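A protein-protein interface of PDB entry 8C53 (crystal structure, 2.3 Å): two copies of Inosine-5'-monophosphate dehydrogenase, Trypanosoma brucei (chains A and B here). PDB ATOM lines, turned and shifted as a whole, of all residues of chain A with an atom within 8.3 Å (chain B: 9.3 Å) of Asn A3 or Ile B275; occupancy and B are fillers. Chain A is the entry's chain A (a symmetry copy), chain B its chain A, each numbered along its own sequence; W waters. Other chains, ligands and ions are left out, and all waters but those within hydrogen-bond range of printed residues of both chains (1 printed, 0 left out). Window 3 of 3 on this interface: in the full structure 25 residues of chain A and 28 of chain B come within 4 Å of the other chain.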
ATOM      1  N   ASN A   3     -17.943  -8.560 -18.737  1.00  0.00           N
ATOM      2  CA  ASN A   3     -16.540  -8.201 -18.618  1.00  0.00           C
ATOM      3  C   ASN A   3     -15.764  -9.259 -17.848  1.00  0.00           C
ATOM      4  O   ASN A   3     -14.810  -8.948 -17.126  1.00  0.00           O
ATOM      5  CB  ASN A   3     -16.378  -6.856 -17.907  1.00  0.00           C
ATOM      6  CG  ASN A   3     -17.013  -5.716 -18.667  1.00  0.00           C
ATOM      7  OD1 ASN A   3     -17.056  -5.725 -19.897  1.00  0.00           O
ATOM      8  ND2 ASN A   3     -17.508  -4.719 -17.935  1.00  0.00           N
ATOM      9  N   THR A   4     -16.171 -10.515 -18.005  1.00  0.00           N
ATOM     10  CA  THR A   4     -15.535 -11.578 -17.238  1.00  0.00           C
ATOM     11  C   THR A   4     -14.091 -11.775 -17.660  1.00  0.00           C
ATOM     12  O   THR A   4     -13.231 -12.064 -16.824  1.00  0.00           O
ATOM     13  CB  THR A   4     -16.324 -12.870 -17.398  1.00  0.00           C
ATOM     14  OG1 THR A   4     -17.728 -12.564 -17.352  1.00  0.00           O
ATOM     15  CG2 THR A   4     -15.982 -13.829 -16.281  1.00  0.00           C
ATOM     16  N   ASN A   5     -13.799 -11.614 -18.948  1.00  0.00           N
ATOM     17  CA  ASN A   5     -12.424 -11.759 -19.401  1.00  0.00           C
ATOM     18  C   ASN A   5     -11.522 -10.720 -18.748  1.00  0.00           C
ATOM     19  O   ASN A   5     -10.332 -10.985 -18.516  1.00  0.00           O
ATOM     20  CB  ASN A   5     -12.359 -11.638 -20.918  1.00  0.00           C
ATOM     21  CG  ASN A   5     -12.155 -12.972 -21.590  1.00  0.00           C
ATOM     22  OD1 ASN A   5     -11.020 -13.470 -21.691  1.00  0.00           O
ATOM     23  ND2 ASN A   5     -13.256 -13.579 -22.053  1.00  0.00           N
ATOM     24  N   LEU A   6     -12.066  -9.535 -18.447  1.00  0.00           N
ATOM     25  CA  LEU A   6     -11.252  -8.485 -17.851  1.00  0.00           C
ATOM     26  C   LEU A   6     -11.161  -8.608 -16.339  1.00  0.00           C
ATOM     27  O   LEU A   6     -10.144  -8.210 -15.753  1.00  0.00           O
ATOM     28  CB  LEU A   6     -11.819  -7.111 -18.219  1.00  0.00           C
ATOM     29  CG  LEU A   6     -11.807  -6.735 -19.698  1.00  0.00           C
ATOM     30  CD1 LEU A   6     -12.828  -5.642 -19.967  1.00  0.00           C
ATOM     31  CD2 LEU A   6     -10.425  -6.289 -20.143  1.00  0.00           C
ATOM     32  N   ARG A   7     -12.197  -9.126 -15.689  1.00  0.00           N
ATOM     33  CA  ARG A   7     -12.197  -9.194 -14.239  1.00  0.00           C
ATOM     34  C   ARG A   7     -11.502 -10.435 -13.707  1.00  0.00           C
ATOM     35  O   ARG A   7     -10.824 -10.373 -12.675  1.00  0.00           O
ATOM     36  CB  ARG A   7     -13.628  -9.160 -13.690  1.00  0.00           C
ATOM     37  CG  ARG A   7     -13.712  -9.533 -12.227  1.00  0.00           C
ATOM     38  CD  ARG A   7     -15.012  -9.076 -11.572  1.00  0.00           C
ATOM     39  NE  ARG A   7     -15.064  -7.627 -11.428  1.00  0.00           N
ATOM     40  CZ  ARG A   7     -15.848  -6.827 -12.148  1.00  0.00           C
ATOM     41  NH1 ARG A   7     -16.675  -7.309 -13.068  1.00  0.00           N
ATOM     42  NH2 ARG A   7     -15.803  -5.511 -11.942  1.00  0.00           N
ATOM     43  N   THR A   8     -11.636 -11.568 -14.394  1.00  0.00           N
ATOM     44  CA  THR A   8     -11.067 -12.806 -13.874  1.00  0.00           C
ATOM     45  C   THR A   8      -9.552 -12.783 -14.046  1.00  0.00           C
ATOM     46  O   THR A   8      -9.047 -12.529 -15.145  1.00  0.00           O
ATOM     47  CB  THR A   8     -11.673 -14.015 -14.577  1.00  0.00           C
ATOM     48  OG1 THR A   8     -11.330 -13.983 -15.964  1.00  0.00           O
ATOM     49  CG2 THR A   8     -13.185 -14.017 -14.408  1.00  0.00           C
ATOM     50  N   PHE A  37     -10.588  -5.196 -10.862  1.00  0.00           N
ATOM     51  CA  PHE A  37     -11.126  -4.562 -12.056  1.00  0.00           C
ATOM     52  C   PHE A  37     -12.430  -3.855 -11.731  1.00  0.00           C
ATOM     53  O   PHE A  37     -13.284  -4.412 -11.041  1.00  0.00           O
ATOM     54  CB  PHE A  37     -11.367  -5.600 -13.156  1.00  0.00           C
ATOM     55  CG  PHE A  37     -12.003  -5.037 -14.383  1.00  0.00           C
ATOM     56  CD1 PHE A  37     -11.242  -4.353 -15.317  1.00  0.00           C
ATOM     57  CD2 PHE A  37     -13.356  -5.173 -14.599  1.00  0.00           C
ATOM     58  CE1 PHE A  37     -11.829  -3.827 -16.451  1.00  0.00           C
ATOM     59  CE2 PHE A  37     -13.947  -4.643 -15.730  1.00  0.00           C
ATOM     60  CZ  PHE A  37     -13.185  -3.973 -16.652  1.00  0.00           C
ATOM     61  N   ILE A  38     -12.604  -2.650 -12.271  1.00  0.00           N
ATOM     62  CA  ILE A  38     -13.720  -1.777 -11.923  1.00  0.00           C
ATOM     63  C   ILE A  38     -14.584  -1.546 -13.156  1.00  0.00           C
ATOM     64  O   ILE A  38     -14.081  -1.117 -14.204  1.00  0.00           O
ATOM     65  CB  ILE A  38     -13.233  -0.427 -11.363  1.00  0.00           C
ATOM     66  CG1 ILE A  38     -12.418  -0.625 -10.089  1.00  0.00           C
ATOM     67  CG2 ILE A  38     -14.419   0.485 -11.092  1.00  0.00           C
ATOM     68  CD1 ILE A  38     -11.534   0.545  -9.754  1.00  0.00           C
ATOM     69  N   ASP A  39     -15.879  -1.841 -13.034  1.00  0.00           N
ATOM     70  CA  ASP A  39     -16.841  -1.510 -14.080  1.00  0.00           C
ATOM     71  C   ASP A  39     -18.152  -1.034 -13.475  1.00  0.00           C
ATOM     72  O   ASP A  39     -19.222  -1.271 -14.041  1.00  0.00           O
ATOM     73  CB  ASP A  39     -17.088  -2.696 -15.016  1.00  0.00           C
ATOM     74  CG  ASP A  39     -17.661  -3.891 -14.304  1.00  0.00           C
ATOM     75  OD1 ASP A  39     -17.772  -3.849 -13.066  1.00  0.00           O
ATOM     76  OD2 ASP A  39     -18.001  -4.884 -14.983  1.00  0.00           O
ATOM     77  N   PHE A  40     -18.088  -0.358 -12.337  1.00  0.00           N
ATOM     78  CA  PHE A  40     -19.289   0.094 -11.657  1.00  0.00           C
ATOM     79  C   PHE A  40     -18.938   1.269 -10.765  1.00  0.00           C
ATOM     80  O   PHE A  40     -17.775   1.470 -10.403  1.00  0.00           O
ATOM     81  CB  PHE A  40     -19.907  -1.029 -10.829  1.00  0.00           C
ATOM     82  CG  PHE A  40     -18.967  -1.615  -9.822  1.00  0.00           C
ATOM     83  CD1 PHE A  40     -18.119  -2.655 -10.171  1.00  0.00           C
ATOM     84  CD2 PHE A  40     -18.914  -1.119  -8.532  1.00  0.00           C
ATOM     85  CE1 PHE A  40     -17.243  -3.195  -9.244  1.00  0.00           C
ATOM     86  CE2 PHE A  40     -18.039  -1.656  -7.607  1.00  0.00           C
ATOM     87  CZ  PHE A  40     -17.211  -2.697  -7.968  1.00  0.00           C
ATOM     88  N   THR B 246     -10.291   9.821 -17.533  1.00  0.00           N
ATOM     89  CA  THR B 246     -10.827   8.948 -18.573  1.00  0.00           C
ATOM     90  C   THR B 246     -12.337   9.083 -18.723  1.00  0.00           C
ATOM     91  O   THR B 246     -12.981   8.201 -19.298  1.00  0.00           O
ATOM     92  CB  THR B 246     -10.476   7.489 -18.290  1.00  0.00           C
ATOM     93  OG1 THR B 246     -11.127   7.065 -17.083  1.00  0.00           O
ATOM     94  CG2 THR B 246      -8.976   7.319 -18.147  1.00  0.00           C
ATOM     95  N   ARG B 247     -12.914  10.163 -18.206  1.00  0.00           N
ATOM     96  CA  ARG B 247     -14.334  10.413 -18.401  1.00  0.00           C
ATOM     97  C   ARG B 247     -14.614  10.808 -19.852  1.00  0.00           C
ATOM     98  O   ARG B 247     -13.715  11.174 -20.617  1.00  0.00           O
ATOM     99  CB  ARG B 247     -14.823  11.510 -17.455  1.00  0.00           C
ATOM    100  CG  ARG B 247     -14.854  11.092 -16.000  1.00  0.00           C
ATOM    101  CD  ARG B 247     -14.953  12.303 -15.071  1.00  0.00           C
ATOM    102  NE  ARG B 247     -14.018  13.354 -15.450  1.00  0.00           N
ATOM    103  CZ  ARG B 247     -14.371  14.588 -15.795  1.00  0.00           C
ATOM    104  NH1 ARG B 247     -15.639  14.971 -15.792  1.00  0.00           N
ATOM    105  NH2 ARG B 247     -13.428  15.458 -16.153  1.00  0.00           N
ATOM    106  N   GLU B 248     -15.893  10.737 -20.225  1.00  0.00           N
ATOM    107  CA  GLU B 248     -16.291  11.111 -21.579  1.00  0.00           C
ATOM    108  C   GLU B 248     -16.011  12.584 -21.855  1.00  0.00           C
ATOM    109  O   GLU B 248     -15.613  12.948 -22.969  1.00  0.00           O
ATOM    110  CB  GLU B 248     -17.766  10.799 -21.791  1.00  0.00           C
ATOM    111  CG  GLU B 248     -18.041   9.314 -21.943  1.00  0.00           C
ATOM    112  CD  GLU B 248     -17.514   8.762 -23.250  1.00  0.00           C
ATOM    113  OE1 GLU B 248     -16.728   7.783 -23.217  1.00  0.00           O
ATOM    114  OE2 GLU B 248     -17.887   9.306 -24.316  1.00  0.00           O
ATOM    115  N   SER B 269      -5.536   8.367 -12.742  1.00  0.00           N
ATOM    116  CA  SER B 269      -6.442   7.528 -11.979  1.00  0.00           C
ATOM    117  C   SER B 269      -5.643   6.838 -10.885  1.00  0.00           C
ATOM    118  O   SER B 269      -4.515   6.400 -11.112  1.00  0.00           O
ATOM    119  CB  SER B 269      -7.127   6.505 -12.884  1.00  0.00           C
ATOM    120  OG  SER B 269      -7.436   5.331 -12.162  1.00  0.00           O
ATOM    121  N   GLN B 271      -6.683   4.025  -9.634  1.00  0.00           N
ATOM    122  CA  GLN B 271      -6.868   2.600  -9.945  1.00  0.00           C
ATOM    123  C   GLN B 271      -7.296   2.539 -11.405  1.00  0.00           C
ATOM    124  O   GLN B 271      -8.478   2.676 -11.714  1.00  0.00           O
ATOM    125  CB  GLN B 271      -7.894   1.960  -9.033  1.00  0.00           C
ATOM    126  CG  GLN B 271      -7.565   0.543  -8.643  1.00  0.00           C
ATOM    127  CD  GLN B 271      -7.978  -0.457  -9.703  1.00  0.00           C
ATOM    128  OE1 GLN B 271      -7.436  -0.468 -10.816  1.00  0.00           O
ATOM    129  NE2 GLN B 271      -8.938  -1.309  -9.363  1.00  0.00           N
ATOM    130  N   GLY B 272      -6.335   2.342 -12.291  1.00  0.00           N
ATOM    131  CA  GLY B 272      -6.572   2.446 -13.710  1.00  0.00           C
ATOM    132  C   GLY B 272      -7.089   1.211 -14.407  1.00  0.00           C
ATOM    133  O   GLY B 272      -7.271   1.235 -15.631  1.00  0.00           O
ATOM    134  N   ASN B 273      -7.311   0.120 -13.685  1.00  0.00           N
ATOM    135  CA  ASN B 273      -7.831  -1.111 -14.289  1.00  0.00           C
ATOM    136  C   ASN B 273      -9.360  -1.054 -14.289  1.00  0.00           C
ATOM    137  O   ASN B 273     -10.047  -1.731 -13.528  1.00  0.00           O
ATOM    138  CB  ASN B 273      -7.307  -2.337 -13.545  1.00  0.00           C
ATOM    139  CG  ASN B 273      -7.666  -3.640 -14.238  1.00  0.00           C
ATOM    140  OD1 ASN B 273      -7.768  -3.694 -15.451  1.00  0.00           O
ATOM    141  ND2 ASN B 273      -7.861  -4.696 -13.457  1.00  0.00           N
ATOM    142  N   THR B 274      -9.883  -0.207 -15.167  1.00  0.00           N
ATOM    143  CA  THR B 274     -11.309   0.069 -15.240  1.00  0.00           C
ATOM    144  C   THR B 274     -11.791  -0.053 -16.672  1.00  0.00           C
ATOM    145  O   THR B 274     -11.024   0.127 -17.616  1.00  0.00           O
ATOM    146  CB  THR B 274     -11.652   1.487 -14.734  1.00  0.00           C
ATOM    147  OG1 THR B 274     -11.558   2.408 -15.830  1.00  0.00           O
ATOM    148  CG2 THR B 274     -10.700   1.918 -13.621  1.00  0.00           C
ATOM    149  N   ILE B 275     -13.080  -0.343 -16.827  1.00  0.00           N
ATOM    150  CA  ILE B 275     -13.665  -0.397 -18.164  1.00  0.00           C
ATOM    151  C   ILE B 275     -13.608   0.979 -18.805  1.00  0.00           C
ATOM    152  O   ILE B 275     -13.420   1.109 -20.024  1.00  0.00           O
ATOM    153  CB  ILE B 275     -15.106  -0.937 -18.099  1.00  0.00           C
ATOM    154  CG1 ILE B 275     -15.586  -1.315 -19.497  1.00  0.00           C
ATOM    155  CG2 ILE B 275     -16.024   0.077 -17.478  1.00  0.00           C
ATOM    156  CD1 ILE B 275     -14.863  -2.496 -20.087  1.00  0.00           C
ATOM    157  N   TYR B 276     -13.772   2.028 -18.000  1.00  0.00           N
ATOM    158  CA  TYR B 276     -13.701   3.381 -18.533  1.00  0.00           C
ATOM    159  C   TYR B 276     -12.333   3.660 -19.122  1.00  0.00           C
ATOM    160  O   TYR B 276     -12.228   4.192 -20.234  1.00  0.00           O
ATOM    161  CB  TYR B 276     -14.040   4.379 -17.431  1.00  0.00           C
ATOM    162  CG  TYR B 276     -15.190   3.910 -16.561  1.00  0.00           C
ATOM    163  CD1 TYR B 276     -16.479   3.843 -17.064  1.00  0.00           C
ATOM    164  CD2 TYR B 276     -14.979   3.505 -15.254  1.00  0.00           C
ATOM    165  CE1 TYR B 276     -17.532   3.413 -16.286  1.00  0.00           C
ATOM    166  CE2 TYR B 276     -16.026   3.066 -14.458  1.00  0.00           C
ATOM    167  CZ  TYR B 276     -17.304   3.018 -14.985  1.00  0.00           C
ATOM    168  OH  TYR B 276     -18.372   2.582 -14.216  1.00  0.00           O
ATOM    169  N   GLN B 277     -11.272   3.266 -18.417  1.00  0.00           N
ATOM    170  CA  GLN B 277      -9.930   3.535 -18.925  1.00  0.00           C
ATOM    171  C   GLN B 277      -9.611   2.663 -20.132  1.00  0.00           C
ATOM    172  O   GLN B 277      -8.943   3.108 -21.064  1.00  0.00           O
ATOM    173  CB  GLN B 277      -8.876   3.338 -17.829  1.00  0.00           C
ATOM    174  CG  GLN B 277      -7.458   3.574 -18.349  1.00  0.00           C
ATOM    175  CD  GLN B 277      -6.465   4.028 -17.295  1.00  0.00           C
ATOM    176  OE1 GLN B 277      -5.279   3.729 -17.408  1.00  0.00           O
ATOM    177  NE2 GLN B 277      -6.938   4.770 -16.279  1.00  0.00           N
ATOM    178  N   VAL B 278     -10.064   1.412 -20.134  1.00  0.00           N
ATOM    179  CA  VAL B 278      -9.831   0.546 -21.294  1.00  0.00           C
ATOM    180  C   VAL B 278     -10.481   1.146 -22.536  1.00  0.00           C
ATOM    181  O   VAL B 278      -9.856   1.253 -23.602  1.00  0.00           O
ATOM    182  CB  VAL B 278     -10.357  -0.876 -21.013  1.00  0.00           C
ATOM    183  CG1 VAL B 278     -10.425  -1.696 -22.303  1.00  0.00           C
ATOM    184  CG2 VAL B 278      -9.475  -1.567 -19.976  1.00  0.00           C
ATOM    185  N   SER B 279     -11.751   1.551 -22.413  1.00  0.00           N
ATOM    186  CA  SER B 279     -12.428   2.190 -23.532  1.00  0.00           C
ATOM    187  C   SER B 279     -11.719   3.472 -23.941  1.00  0.00           C
ATOM    188  O   SER B 279     -11.584   3.757 -25.134  1.00  0.00           O
ATOM    189  CB  SER B 279     -13.876   2.486 -23.165  1.00  0.00           C
ATOM    190  OG  SER B 279     -14.499   1.306 -22.697  1.00  0.00           O
ATOM    191  N   PHE B 280     -11.275   4.266 -22.966  1.00  0.00           N
ATOM    192  CA  PHE B 280     -10.596   5.514 -23.289  1.00  0.00           C
ATOM    193  C   PHE B 280      -9.310   5.259 -24.058  1.00  0.00           C
ATOM    194  O   PHE B 280      -9.006   5.965 -25.024  1.00  0.00           O
ATOM    195  CB  PHE B 280     -10.305   6.291 -22.009  1.00  0.00           C
ATOM    196  CG  PHE B 280     -10.182   7.762 -22.217  1.00  0.00           C
ATOM    197  CD1 PHE B 280     -11.308   8.556 -22.336  1.00  0.00           C
ATOM    198  CD2 PHE B 280      -8.938   8.357 -22.294  1.00  0.00           C
ATOM    199  CE1 PHE B 280     -11.194   9.914 -22.532  1.00  0.00           C
ATOM    200  CE2 PHE B 280      -8.819   9.724 -22.493  1.00  0.00           C
ATOM    201  CZ  PHE B 280      -9.949  10.503 -22.606  1.00  0.00           C
ATOM    202  N   ILE B 281      -8.527   4.269 -23.635  1.00  0.00           N
ATOM    203  CA  ILE B 281      -7.294   3.958 -24.348  1.00  0.00           C
ATOM    204  C   ILE B 281      -7.609   3.503 -25.764  1.00  0.00           C
ATOM    205  O   ILE B 281      -6.963   3.931 -26.729  1.00  0.00           O
ATOM    206  CB  ILE B 281      -6.480   2.891 -23.604  1.00  0.00           C
ATOM    207  CG1 ILE B 281      -6.005   3.396 -22.250  1.00  0.00           C
ATOM    208  CG2 ILE B 281      -5.271   2.489 -24.429  1.00  0.00           C
ATOM    209  CD1 ILE B 281      -5.403   2.297 -21.389  1.00  0.00           C
ATOM    210  N   ARG B 282      -8.606   2.627 -25.910  1.00  0.00           N
ATOM    211  CA  ARG B 282      -9.009   2.187 -27.241  1.00  0.00           C
ATOM    212  C   ARG B 282      -9.376   3.384 -28.107  1.00  0.00           C
ATOM    213  O   ARG B 282      -8.908   3.515 -29.245  1.00  0.00           O
ATOM    214  CB  ARG B 282     -10.180   1.207 -27.134  1.00  0.00           C
ATOM    215  CG  ARG B 282      -9.769  -0.251 -26.914  1.00  0.00           C
ATOM    216  CD  ARG B 282     -10.910  -1.105 -26.351  1.00  0.00           C
ATOM    217  NE  ARG B 282     -10.421  -2.378 -25.828  1.00  0.00           N
ATOM    218  CZ  ARG B 282     -11.151  -3.254 -25.146  1.00  0.00           C
ATOM    219  NH1 ARG B 282     -12.439  -3.051 -24.914  1.00  0.00           N
ATOM    220  NH2 ARG B 282     -10.571  -4.357 -24.677  1.00  0.00           N
ATOM    221  N   TRP B 283     -10.187   4.291 -27.565  1.00  0.00           N
ATOM    222  CA  TRP B 283     -10.643   5.444 -28.329  1.00  0.00           C
ATOM    223  C   TRP B 283      -9.492   6.364 -28.717  1.00  0.00           C
ATOM    224  O   TRP B 283      -9.443   6.862 -29.848  1.00  0.00           O
ATOM    225  CB  TRP B 283     -11.674   6.226 -27.521  1.00  0.00           C
ATOM    226  CG  TRP B 283     -12.067   7.509 -28.167  1.00  0.00           C
ATOM    227  CD1 TRP B 283     -13.046   7.690 -29.094  1.00  0.00           C
ATOM    228  CD2 TRP B 283     -11.488   8.799 -27.936  1.00  0.00           C
ATOM    229  NE1 TRP B 283     -13.114   9.018 -29.457  1.00  0.00           N
ATOM    230  CE2 TRP B 283     -12.163   9.716 -28.763  1.00  0.00           C
ATOM    231  CE3 TRP B 283     -10.465   9.267 -27.109  1.00  0.00           C
ATOM    232  CZ2 TRP B 283     -11.851  11.066 -28.784  1.00  0.00           C
ATOM    233  CZ3 TRP B 283     -10.156  10.611 -27.135  1.00  0.00           C
ATOM    234  CH2 TRP B 283     -10.846  11.493 -27.968  1.00  0.00           C
ATOM    235  N   ASN B 306      -4.665  -6.005 -18.624  1.00  0.00           N
ATOM    236  CA  ASN B 306      -5.844  -5.391 -19.225  1.00  0.00           C
ATOM    237  C   ASN B 306      -5.467  -4.115 -19.964  1.00  0.00           C
ATOM    238  O   ASN B 306      -5.902  -3.890 -21.103  1.00  0.00           O
ATOM    239  CB  ASN B 306      -6.905  -5.096 -18.165  1.00  0.00           C
ATOM    240  CG  ASN B 306      -7.739  -6.317 -17.820  1.00  0.00           C
ATOM    241  OD1 ASN B 306      -7.797  -7.281 -18.587  1.00  0.00           O
ATOM    242  ND2 ASN B 306      -8.388  -6.283 -16.654  1.00  0.00           N
ATOM    243  N   LEU B 307      -4.625  -3.271 -19.342  1.00  0.00           N
ATOM    244  CA  LEU B 307      -4.323  -1.968 -19.940  1.00  0.00           C
ATOM    245  C   LEU B 307      -3.393  -2.086 -21.146  1.00  0.00           C
ATOM    246  O   LEU B 307      -3.482  -1.282 -22.086  1.00  0.00           O
ATOM    247  CB  LEU B 307      -3.715  -1.042 -18.896  1.00  0.00           C
ATOM    248  CG  LEU B 307      -4.639  -0.795 -17.707  1.00  0.00           C
ATOM    249  CD1 LEU B 307      -4.071   0.240 -16.746  1.00  0.00           C
ATOM    250  CD2 LEU B 307      -6.021  -0.356 -18.204  1.00  0.00           C
ATOM    251  N   ALA B 310      -5.544  -3.180 -23.999  1.00  0.00           N
ATOM    252  CA  ALA B 310      -6.273  -2.045 -24.555  1.00  0.00           C
ATOM    253  C   ALA B 310      -5.416  -1.223 -25.514  1.00  0.00           C
ATOM    254  O   ALA B 310      -5.964  -0.514 -26.364  1.00  0.00           O
ATOM    255  CB  ALA B 310      -6.796  -1.147 -23.439  1.00  0.00           C
HETATM  256  O   HOH W   1      -7.887  -7.622 -13.483  1.00  0.00           O
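The backbone carbonyl oxygen (O) of Gln B271 is in hydrogen-bond range of the side-chain hydroxyl (OG) of Ser B269 (2.9 Å).
The side-chain amide oxygen (OD1) of Asn B273 is in hydrogen-bond range of the side-chain amide nitrogen (ND2) of Asn B306, 2.9 Å away.
OG1 of Thr B274 lies within hydrogen-bond range of N of Tyr B276 (3.1 Å).
OG1 of Thr B274 is in hydrogen-bond range of N of Gln B277 (2.7 Å).
The guanidinium group (NH2) of Arg A7 sits at hydrogen-bond distance from the backbone carbonyl oxygen (O) of Phe A37, at 2.9 Å.
NH2 of Arg A7 is in salt-bridge range of OD1 of Asp A39 (2.8 Å).
No position is printed for both chains.
The backbone carbonyl oxygen (O) of Asn B273 sits at hydrogen-bond distance from the backbone NH (N) of Ile A38, 3.0 Å away.
The backbone carbonyl oxygen (O) of Ile A38 is in hydrogen-bond range of the backbone NH (N) of Ile B275, 2.9 Å away.
The side-chain amide nitrogen (ND2) of Asn B306 lies within hydrogen-bond range of the backbone carbonyl oxygen (O) of Leu A6 (2.8 Å).
Hydrophobic or aromatic side chains of chain B within 4 Å of the printed part of chain A: Ile B275 and Tyr B276.
Along chain B the printed residues that touch a printed residue of chain A span positions 271 to 306.
Of the 10 printed residues of chain A, 6 touch a printed residue of chain B.
Hydrophobic or aromatic side chains of chain A within 4 Å of the printed part of chain B: Leu A6, Phe A37 and Ile A38.
Among the printed residues, 14 pairs touch across the chains.
Among the printed residues, no Asp or Glu carboxylate lies within 4 Å of a Lys or Arg side-chain nitrogen of the other chain.
Among the printed residues, merely in contact across the chains: Asn A3 with Ile B275, Leu A6 with Ile B275, Phe A37 with Asn B273, Phe A37 with Thr B274, Phe A37 with Ile B275, Phe A37 with Asn B306, Ile A38 with Gln B271, Ile A38 with Thr B274, Asp A39 with Ile B275, Asp A39 with Tyr B276 and Phe A40 with Tyr B276.
Water W1 lies within hydrogen-bond range of the side-chain amide nitrogen (ND2) of Asn B273, the backbone carbonyl oxygen (O) of Leu A6 and the side-chain amide nitrogen (ND2) of Asn B306.
Asn A3 touches just one residue of chain B: Ile B275.
Ile B275 touches just these residues of chain A: Asn A3 (3.9 Å), Leu A6 (3.7 Å), Phe A37 (3.6 Å), Ile A38 (2.9 Å) and Asp A39 (3.8 Å).
Thr A4 touches none of the printed residues of chain B.
Printed residues of chain B within 4 Å of Asp A39: Ile B275 and Tyr B276.
Printed residues of chain B within 4 Å of Phe A37: Asn B273 (3.4 Å), Thr B274 (3.8 Å), Ile B275 (3.6 Å) and Asn B306 (3.7 Å).
Printed residues of chain A within 4 Å of Asn B306: Leu A6 and Phe A37.
Printed residues of chain A within 4 Å of Asn B273: Phe A37 (3.4 Å) and Ile A38 (3.0 Å).
Printed residues of chain A within 4 Å of Thr B274: Phe A37 (3.8 Å) and Ile A38 (3.2 Å).
The nearest printed residue of chain B that does not touch Phe A40 is Ile B275 (5.6 Å).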
